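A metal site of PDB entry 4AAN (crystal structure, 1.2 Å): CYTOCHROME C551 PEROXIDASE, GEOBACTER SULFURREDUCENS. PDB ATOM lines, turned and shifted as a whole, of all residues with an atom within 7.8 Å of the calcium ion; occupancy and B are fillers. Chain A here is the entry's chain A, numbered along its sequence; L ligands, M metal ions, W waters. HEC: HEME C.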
ATOM      1  N   THR A  79      -1.019   1.443  -7.560  1.00  0.00           N
ATOM      2  CA  THR A  79      -1.616   0.340  -6.805  1.00  0.00           C
ATOM      3  C   THR A  79      -3.123   0.359  -7.028  1.00  0.00           C
ATOM      4  O   THR A  79      -3.575   1.091  -7.921  1.00  0.00           O
ATOM      5  CB  THR A  79      -1.214   0.358  -5.228  1.00  0.00           C
ATOM      6  OG1 THR A  79      -1.831  -0.725  -4.507  1.00  0.00           O
ATOM      7  CG2 THR A  79      -1.530   1.663  -4.528  1.00  0.00           C
ATOM      8  N   ASP A  80      -3.892  -0.483  -6.345  1.00  0.00           N
ATOM      9  CA  ASP A  80      -5.337  -0.570  -6.576  1.00  0.00           C
ATOM     10  C   ASP A  80      -6.096  -0.139  -5.341  1.00  0.00           C
ATOM     11  O   ASP A  80      -7.347  -0.214  -5.366  1.00  0.00           O
ATOM     12  CB  ASP A  80      -5.748  -2.022  -6.959  1.00  0.00           C
ATOM     13  CG  ASP A  80      -5.352  -3.009  -5.955  1.00  0.00           C
ATOM     14  OD1 ASP A  80      -4.980  -2.760  -4.842  1.00  0.00           O
ATOM     15  OD2 ASP A  80      -5.410  -4.267  -6.334  1.00  0.00           O
ATOM     16  N   ILE A  81      -5.446   0.284  -4.278  1.00  0.00           N
ATOM     17  CA  ILE A  81      -6.124   0.799  -3.029  1.00  0.00           C
ATOM     18  C   ILE A  81      -7.098  -0.166  -2.483  1.00  0.00           C
ATOM     19  O   ILE A  81      -8.097   0.227  -1.837  1.00  0.00           O
ATOM     20  CB  ILE A  81      -6.615   2.268  -3.150  1.00  0.00           C
ATOM     21  CG1 ILE A  81      -7.707   2.417  -4.226  1.00  0.00           C
ATOM     22  CG2 ILE A  81      -5.456   3.201  -3.486  1.00  0.00           C
ATOM     23  CD1 ILE A  81      -8.390   3.812  -4.197  1.00  0.00           C
ATOM     24  N   LEU A  82      -6.816  -1.482  -2.616  1.00  0.00           N
ATOM     25  CA  LEU A  82      -7.599  -2.532  -1.979  1.00  0.00           C
ATOM     26  C   LEU A  82      -6.732  -3.206  -0.947  1.00  0.00           C
ATOM     27  O   LEU A  82      -5.485  -3.218  -1.049  1.00  0.00           O
ATOM     28  CB  LEU A  82      -8.043  -3.621  -2.994  1.00  0.00           C
ATOM     29  CG  LEU A  82      -8.769  -3.072  -4.227  1.00  0.00           C
ATOM     30  CD1 LEU A  82      -9.266  -4.318  -5.062  1.00  0.00           C
ATOM     31  CD2 LEU A  82      -9.946  -2.213  -3.910  1.00  0.00           C
ATOM     32  N   GLU A  83      -7.334  -3.936   0.032  1.00  0.00           N
ATOM     33  CA  GLU A  83      -6.541  -4.760   0.929  1.00  0.00           C
ATOM     34  C   GLU A  83      -5.701  -5.767   0.169  1.00  0.00           C
ATOM     35  O   GLU A  83      -4.475  -5.835   0.333  1.00  0.00           O
ATOM     36  CB  GLU A  83      -7.439  -5.473   1.963  1.00  0.00           C
ATOM     37  CG  GLU A  83      -8.045  -4.443   2.902  1.00  0.00           C
ATOM     38  CD  GLU A  83      -8.689  -5.045   4.108  1.00  0.00           C
ATOM     39  OE1 GLU A  83      -8.691  -6.282   4.366  1.00  0.00           O
ATOM     40  OE2 GLU A  83      -9.155  -4.220   4.940  1.00  0.00           O
ATOM     41  N   ASN A  96      -1.428  -7.637  -0.883  1.00  0.00           N
ATOM     42  CA  ASN A  96      -1.645  -6.287  -1.331  1.00  0.00           C
ATOM     43  C   ASN A  96      -0.807  -5.998  -2.541  1.00  0.00           C
ATOM     44  O   ASN A  96       0.377  -6.396  -2.648  1.00  0.00           O
ATOM     45  CB  ASN A  96      -1.221  -5.360  -0.155  1.00  0.00           C
ATOM     46  CG  ASN A  96      -1.477  -3.894  -0.426  1.00  0.00           C
ATOM     47  OD1 ASN A  96      -0.513  -3.130  -0.651  1.00  0.00           O
ATOM     48  ND2 ASN A  96      -2.743  -3.469  -0.491  1.00  0.00           N
ATOM     49  N   SER A  97      -1.359  -5.218  -3.511  1.00  0.00           N
ATOM     50  CA  SER A  97      -0.519  -4.926  -4.739  1.00  0.00           C
ATOM     51  C   SER A  97       0.437  -3.770  -4.455  1.00  0.00           C
ATOM     52  O   SER A  97       0.064  -2.644  -4.075  1.00  0.00           O
ATOM     53  CB  SER A  97      -1.386  -4.701  -5.972  1.00  0.00           C
ATOM     54  OG  SER A  97      -2.142  -3.545  -5.796  1.00  0.00           O
ATOM     55  N   PRO A  98       1.715  -4.089  -4.518  1.00  0.00           N
ATOM     56  CA  PRO A  98       2.718  -3.046  -4.375  1.00  0.00           C
ATOM     57  C   PRO A  98       2.751  -2.127  -5.570  1.00  0.00           C
ATOM     58  O   PRO A  98       2.327  -2.479  -6.672  1.00  0.00           O
ATOM     59  CB  PRO A  98       4.030  -3.878  -4.273  1.00  0.00           C
ATOM     60  CG  PRO A  98       3.712  -5.071  -5.115  1.00  0.00           C
ATOM     61  CD  PRO A  98       2.292  -5.366  -5.022  1.00  0.00           C
ATOM     62  N   THR A  99       3.263  -0.912  -5.405  1.00  0.00           N
ATOM     63  CA  THR A  99       3.311   0.040  -6.493  1.00  0.00           C
ATOM     64  C   THR A  99       4.325  -0.364  -7.569  1.00  0.00           C
ATOM     65  O   THR A  99       5.427  -0.838  -7.246  1.00  0.00           O
ATOM     66  CB  THR A  99       3.579   1.442  -5.978  1.00  0.00           C
ATOM     67  OG1 THR A  99       3.511   2.335  -7.098  1.00  0.00           O
ATOM     68  CG2 THR A  99       4.951   1.623  -5.300  1.00  0.00           C
ATOM     69  N   TRP A 111       6.709  -9.301  -3.015  1.00  0.00           N
ATOM     70  CA  TRP A 111       6.972  -9.058  -1.594  1.00  0.00           C
ATOM     71  C   TRP A 111       7.963 -10.105  -1.046  1.00  0.00           C
ATOM     72  O   TRP A 111       8.565  -9.819   0.018  1.00  0.00           O
ATOM     73  CB  TRP A 111       5.634  -9.255  -0.806  1.00  0.00           C
ATOM     74  CG  TRP A 111       4.708  -8.090  -0.918  1.00  0.00           C
ATOM     75  CD1 TRP A 111       3.604  -8.007  -1.712  1.00  0.00           C
ATOM     76  CD2 TRP A 111       4.730  -6.914  -0.115  1.00  0.00           C
ATOM     77  NE1 TRP A 111       2.964  -6.791  -1.504  1.00  0.00           N
ATOM     78  CE2 TRP A 111       3.627  -6.116  -0.535  1.00  0.00           C
ATOM     79  CE3 TRP A 111       5.560  -6.466   0.936  1.00  0.00           C
ATOM     80  CZ2 TRP A 111       3.346  -4.848   0.033  1.00  0.00           C
ATOM     81  CZ3 TRP A 111       5.273  -5.205   1.509  1.00  0.00           C
ATOM     82  CH2 TRP A 111       4.192  -4.416   1.049  1.00  0.00           C
ATOM     83  N   VAL A 270       4.644   6.242  -0.243  1.00  0.00           N
ATOM     84  CA  VAL A 270       3.846   5.456   0.717  1.00  0.00           C
ATOM     85  C   VAL A 270       2.607   6.244   1.120  1.00  0.00           C
ATOM     86  O   VAL A 270       1.631   5.523   1.440  1.00  0.00           O
ATOM     87  CB  VAL A 270       4.784   5.110   1.900  1.00  0.00           C
ATOM     88  CG1 VAL A 270       5.179   6.310   2.749  1.00  0.00           C
ATOM     89  CG2 VAL A 270       4.103   4.084   2.756  1.00  0.00           C
ATOM     90  N   ILE A 272       0.433   7.620  -0.512  1.00  0.00           N
ATOM     91  CA  ILE A 272      -0.682   7.463  -1.463  1.00  0.00           C
ATOM     92  C   ILE A 272      -0.903   5.981  -1.877  1.00  0.00           C
ATOM     93  O   ILE A 272      -1.670   5.719  -2.789  1.00  0.00           O
ATOM     94  CB  ILE A 272      -0.517   8.351  -2.686  1.00  0.00           C
ATOM     95  CG1 ILE A 272       0.643   7.913  -3.629  1.00  0.00           C
ATOM     96  CG2 ILE A 272      -0.409   9.811  -2.226  1.00  0.00           C
ATOM     97  CD1 ILE A 272       0.711   8.686  -4.943  1.00  0.00           C
ATOM     98  N   THR A 273      -0.292   5.040  -1.201  1.00  0.00           N
ATOM     99  CA  THR A 273      -0.407   3.591  -1.548  1.00  0.00           C
ATOM    100  C   THR A 273      -0.979   2.696  -0.479  1.00  0.00           C
ATOM    101  O   THR A 273      -0.713   1.497  -0.401  1.00  0.00           O
ATOM    102  CB  THR A 273       0.950   3.018  -2.089  1.00  0.00           C
ATOM    103  OG1 THR A 273       1.888   3.096  -1.004  1.00  0.00           O
ATOM    104  CG2 THR A 273       1.470   3.773  -3.271  1.00  0.00           C
ATOM    105  N   MET A 274      -1.786   3.350   0.384  1.00  0.00           N
ATOM    106  CA  MET A 274      -2.516   2.555   1.358  1.00  0.00           C
ATOM    107  C   MET A 274      -3.381   1.480   0.693  1.00  0.00           C
ATOM    108  O   MET A 274      -3.752   1.588  -0.500  1.00  0.00           O
ATOM    109  CB  MET A 274      -3.449   3.508   2.179  1.00  0.00           C
ATOM    110  CG  MET A 274      -4.636   4.172   1.372  1.00  0.00           C
ATOM    111  SD  MET A 274      -4.088   5.564   0.419  1.00  0.00           S
ATOM    112  CE  MET A 274      -3.989   6.840   1.686  1.00  0.00           C
ATOM    113  N   PRO A 275      -3.828   0.448   1.415  1.00  0.00           N
ATOM    114  CA  PRO A 275      -3.424   0.046   2.749  1.00  0.00           C
ATOM    115  C   PRO A 275      -2.013  -0.562   2.706  1.00  0.00           C
ATOM    116  O   PRO A 275      -1.396  -0.744   1.662  1.00  0.00           O
ATOM    117  CB  PRO A 275      -4.505  -0.927   3.203  1.00  0.00           C
ATOM    118  CG  PRO A 275      -4.956  -1.633   1.899  1.00  0.00           C
ATOM    119  CD  PRO A 275      -4.780  -0.546   0.827  1.00  0.00           C
ATOM    120  N   TYR A 276      -1.524  -0.916   3.883  1.00  0.00           N
ATOM    121  CA  TYR A 276      -0.089  -1.183   4.086  1.00  0.00           C
ATOM    122  C   TYR A 276       0.142  -2.620   4.535  1.00  0.00           C
ATOM    123  O   TYR A 276      -0.736  -3.398   5.036  1.00  0.00           O
ATOM    124  CB  TYR A 276       0.446  -0.200   5.180  1.00  0.00           C
ATOM    125  CG  TYR A 276       0.280   1.220   4.703  1.00  0.00           C
ATOM    126  CD1 TYR A 276       0.932   1.675   3.569  1.00  0.00           C
ATOM    127  CD2 TYR A 276      -0.642   2.085   5.264  1.00  0.00           C
ATOM    128  CE1 TYR A 276       0.758   2.937   3.048  1.00  0.00           C
ATOM    129  CE2 TYR A 276      -0.897   3.352   4.755  1.00  0.00           C
ATOM    130  CZ  TYR A 276      -0.188   3.766   3.659  1.00  0.00           C
ATOM    131  OH  TYR A 276      -0.373   5.057   3.182  1.00  0.00           O
ATOM    132  N   PHE A 277       1.423  -3.013   4.354  1.00  0.00           N
ATOM    133  CA  PHE A 277       2.022  -4.349   4.540  1.00  0.00           C
ATOM    134  C   PHE A 277       1.565  -5.270   3.461  1.00  0.00           C
ATOM    135  O   PHE A 277       0.637  -5.014   2.667  1.00  0.00           O
ATOM    136  CB  PHE A 277       1.831  -4.929   5.985  1.00  0.00           C
ATOM    137  CG  PHE A 277       2.311  -3.947   7.036  1.00  0.00           C
ATOM    138  CD1 PHE A 277       3.579  -3.457   7.017  1.00  0.00           C
ATOM    139  CD2 PHE A 277       1.403  -3.482   8.007  1.00  0.00           C
ATOM    140  CE1 PHE A 277       4.034  -2.521   7.998  1.00  0.00           C
ATOM    141  CE2 PHE A 277       1.868  -2.582   9.031  1.00  0.00           C
ATOM    142  CZ  PHE A 277       3.160  -2.095   8.986  1.00  0.00           C
ATOM    143  N   HIS A 278       2.181  -6.483   3.457  1.00  0.00           N
ATOM    144  CA  HIS A 278       1.888  -7.365   2.325  1.00  0.00           C
ATOM    145  C   HIS A 278       0.450  -7.896   2.461  1.00  0.00           C
ATOM    146  O   HIS A 278      -0.124  -8.420   1.493  1.00  0.00           O
ATOM    147  CB  HIS A 278       2.891  -8.564   2.290  1.00  0.00           C
ATOM    148  CG  HIS A 278       2.708  -9.541   3.490  1.00  0.00           C
ATOM    149  ND1 HIS A 278       3.378  -9.338   4.674  1.00  0.00           N
ATOM    150  CD2 HIS A 278       1.936 -10.668   3.662  1.00  0.00           C
ATOM    151  CE1 HIS A 278       3.039 -10.328   5.537  1.00  0.00           C
ATOM    152  NE2 HIS A 278       2.130 -11.114   4.905  1.00  0.00           N
ATOM    153  N   GLY A 280      -2.110  -5.993   3.508  1.00  0.00           N
ATOM    154  CA  GLY A 280      -3.099  -4.907   3.214  1.00  0.00           C
ATOM    155  C   GLY A 280      -4.069  -4.635   4.312  1.00  0.00           C
ATOM    156  O   GLY A 280      -5.110  -4.066   4.071  1.00  0.00           O
ATOM    157  N   VAL A 282      -3.633  -2.878   7.209  1.00  0.00           N
ATOM    158  CA  VAL A 282      -3.439  -1.674   8.024  1.00  0.00           C
ATOM    159  C   VAL A 282      -3.681  -0.515   7.116  1.00  0.00           C
ATOM    160  O   VAL A 282      -2.836  -0.187   6.244  1.00  0.00           O
ATOM    161  CB  VAL A 282      -2.010  -1.693   8.655  1.00  0.00           C
ATOM    162  CG1 VAL A 282      -1.720  -0.400   9.409  1.00  0.00           C
ATOM    163  CG2 VAL A 282      -1.884  -2.949   9.584  1.00  0.00           C
HETATM  164 FE   HEC L   1       9.545  -0.896   7.842  1.00  0.00          FE
HETATM  165  CHA HEC L   1       7.083  -2.169   5.837  1.00  0.00           C
HETATM  166  CHB HEC L   1       7.890   2.106   7.994  1.00  0.00           C
HETATM  167  CHC HEC L   1      11.515   0.030  10.483  1.00  0.00           C
HETATM  168  CHD HEC L   1      11.450  -3.720   7.388  1.00  0.00           C
HETATM  169  NA  HEC L   1       7.886  -0.167   7.019  1.00  0.00           N
HETATM  170  C1A HEC L   1       6.957  -0.832   6.250  1.00  0.00           C
HETATM  171  C2A HEC L   1       5.855   0.045   5.913  1.00  0.00           C
HETATM  172  C3A HEC L   1       6.122   1.215   6.497  1.00  0.00           C
HETATM  173  C4A HEC L   1       7.355   1.066   7.215  1.00  0.00           C
HETATM  174  CMA HEC L   1       5.271   2.470   6.450  1.00  0.00           C
HETATM  175  CAA HEC L   1       4.688  -0.307   5.018  1.00  0.00           C
HETATM  176  CBA HEC L   1       4.972   0.138   3.570  1.00  0.00           C
HETATM  177  CGA HEC L   1       4.098  -0.497   2.525  1.00  0.00           C
HETATM  178  O1A HEC L   1       4.264  -0.177   1.318  1.00  0.00           O
HETATM  179  O2A HEC L   1       3.237  -1.369   2.890  1.00  0.00           O
HETATM  180  NB  HEC L   1       9.716   0.813   8.993  1.00  0.00           N
HETATM  181  C1B HEC L   1       8.968   1.944   8.877  1.00  0.00           C
HETATM  182  C2B HEC L   1       9.316   2.857   9.910  1.00  0.00           C
HETATM  183  C3B HEC L   1      10.309   2.235  10.667  1.00  0.00           C
HETATM  184  C4B HEC L   1      10.540   0.948  10.077  1.00  0.00           C
HETATM  185  CMB HEC L   1       8.750   4.237  10.078  1.00  0.00           C
HETATM  186  CAB HEC L   1      11.026   2.773  11.911  1.00  0.00           C
HETATM  187  CBB HEC L   1      10.045   3.011  13.001  1.00  0.00           C
HETATM  188  NC  HEC L   1      11.169  -1.663   8.725  1.00  0.00           N
HETATM  189  C1C HEC L   1      11.852  -1.178   9.850  1.00  0.00           C
HETATM  190  C2C HEC L   1      13.011  -1.922  10.115  1.00  0.00           C
HETATM  191  C3C HEC L   1      13.000  -2.950   9.189  1.00  0.00           C
HETATM  192  C4C HEC L   1      11.867  -2.807   8.377  1.00  0.00           C
HETATM  193  CMC HEC L   1      14.006  -1.622  11.202  1.00  0.00           C
HETATM  194  CAC HEC L   1      14.054  -4.009   8.959  1.00  0.00           C
HETATM  195  CBC HEC L   1      14.466  -4.820  10.075  1.00  0.00           C
HETATM  196  ND  HEC L   1       9.324  -2.555   6.780  1.00  0.00           N
HETATM  197  C1D HEC L   1      10.179  -3.628   6.761  1.00  0.00           C
HETATM  198  C2D HEC L   1       9.628  -4.750   6.003  1.00  0.00           C
HETATM  199  C3D HEC L   1       8.403  -4.324   5.613  1.00  0.00           C
HETATM  200  C4D HEC L   1       8.218  -2.968   6.090  1.00  0.00           C
HETATM  201  CMD HEC L   1      10.300  -6.068   5.760  1.00  0.00           C
HETATM  202  CAD HEC L   1       7.331  -5.138   4.929  1.00  0.00           C
HETATM  203  CBD HEC L   1       6.672  -6.084   5.996  1.00  0.00           C
HETATM  204  CGD HEC L   1       5.536  -6.767   5.342  1.00  0.00           C
HETATM  205  O1D HEC L   1       5.546  -8.058   5.357  1.00  0.00           O
HETATM  206  O2D HEC L   1       4.570  -6.172   4.891  1.00  0.00           O
HETATM  207 CA    CA M   1      -0.081  -0.763  -0.256  1.00  0.00          CA
HETATM  208  O   HOH W   1       1.846   0.613   0.302  1.00  0.00           O
HETATM  209  O   HOH W   2       1.431  -2.147   1.039  1.00  0.00           O
HETATM  210  O   HOH W   3       0.896  -0.688  -2.371  1.00  0.00           O
HETATM  211  O   HOH W   4      -2.201  -0.662  -1.563  1.00  0.00           O
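An oxygen (O2A) of the ligand sits at hydrogen-bond distance from the backbone NH (N) of Phe 277 (2.9 Å).
The backbone NH (N) of His 278 sits at hydrogen-bond distance from an oxygen (O2D) of the ligand, 2.8 Å away.
An oxygen (O1D) of the ligand sits at hydrogen-bond distance from a ring nitrogen (ND1) of His 278 (2.6 Å).
The backbone carbonyl oxygen of Val 270 lies within hydrogen-bond range of the side-chain hydroxyl of Thr 273 (3.5 Å).
The backbone carbonyl oxygen of Asn 96 is in hydrogen-bond range of the indole nitrogen of Trp 111.
O of Leu 82 is in hydrogen-bond range of ND2 of Asn 96 (2.8 Å).
The side-chain amide nitrogen (ND2) of Asn 96 is in hydrogen-bond range of the backbone carbonyl oxygen (O) of Glu 83 (3.0 Å).
N of Asn 96 lies within hydrogen-bond range of O of His 278 (2.8 Å).
Three residues have an atom within 4 Å of the calcium ion: Asn 96, Thr 273 and Pro 275.
The calcium ion is bound by O of Pro 275 (2.3 Å), water W3 (2.3 Å), O of Thr 273 (2.4 Å), water W2 (2.4 Å), water W1 (2.4 Å), OD1 of Asn 96 (2.4 Å) and water W4 (2.5 Å).
The calcium ion has seven donor atoms within binding distance.
Water W4 lies within hydrogen-bond range of the backbone carbonyl oxygen of Met 274 (2.9 Å), the side-chain hydroxyl of Thr 79 (3.0 Å) and the side-chain amide nitrogen of Asn 96 (3.1 Å).
Water W3 lies within hydrogen-bond range of O of Ser 97 and OG1 of Thr 79.
Water W1 bridges O1A of the ligand (2.7 Å) and OG1 of Thr 273 (2.8 Å).
Water W2 lies within hydrogen-bond range of O2A of the ligand (2.7 Å) and O of Phe 277 (3.4 Å).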
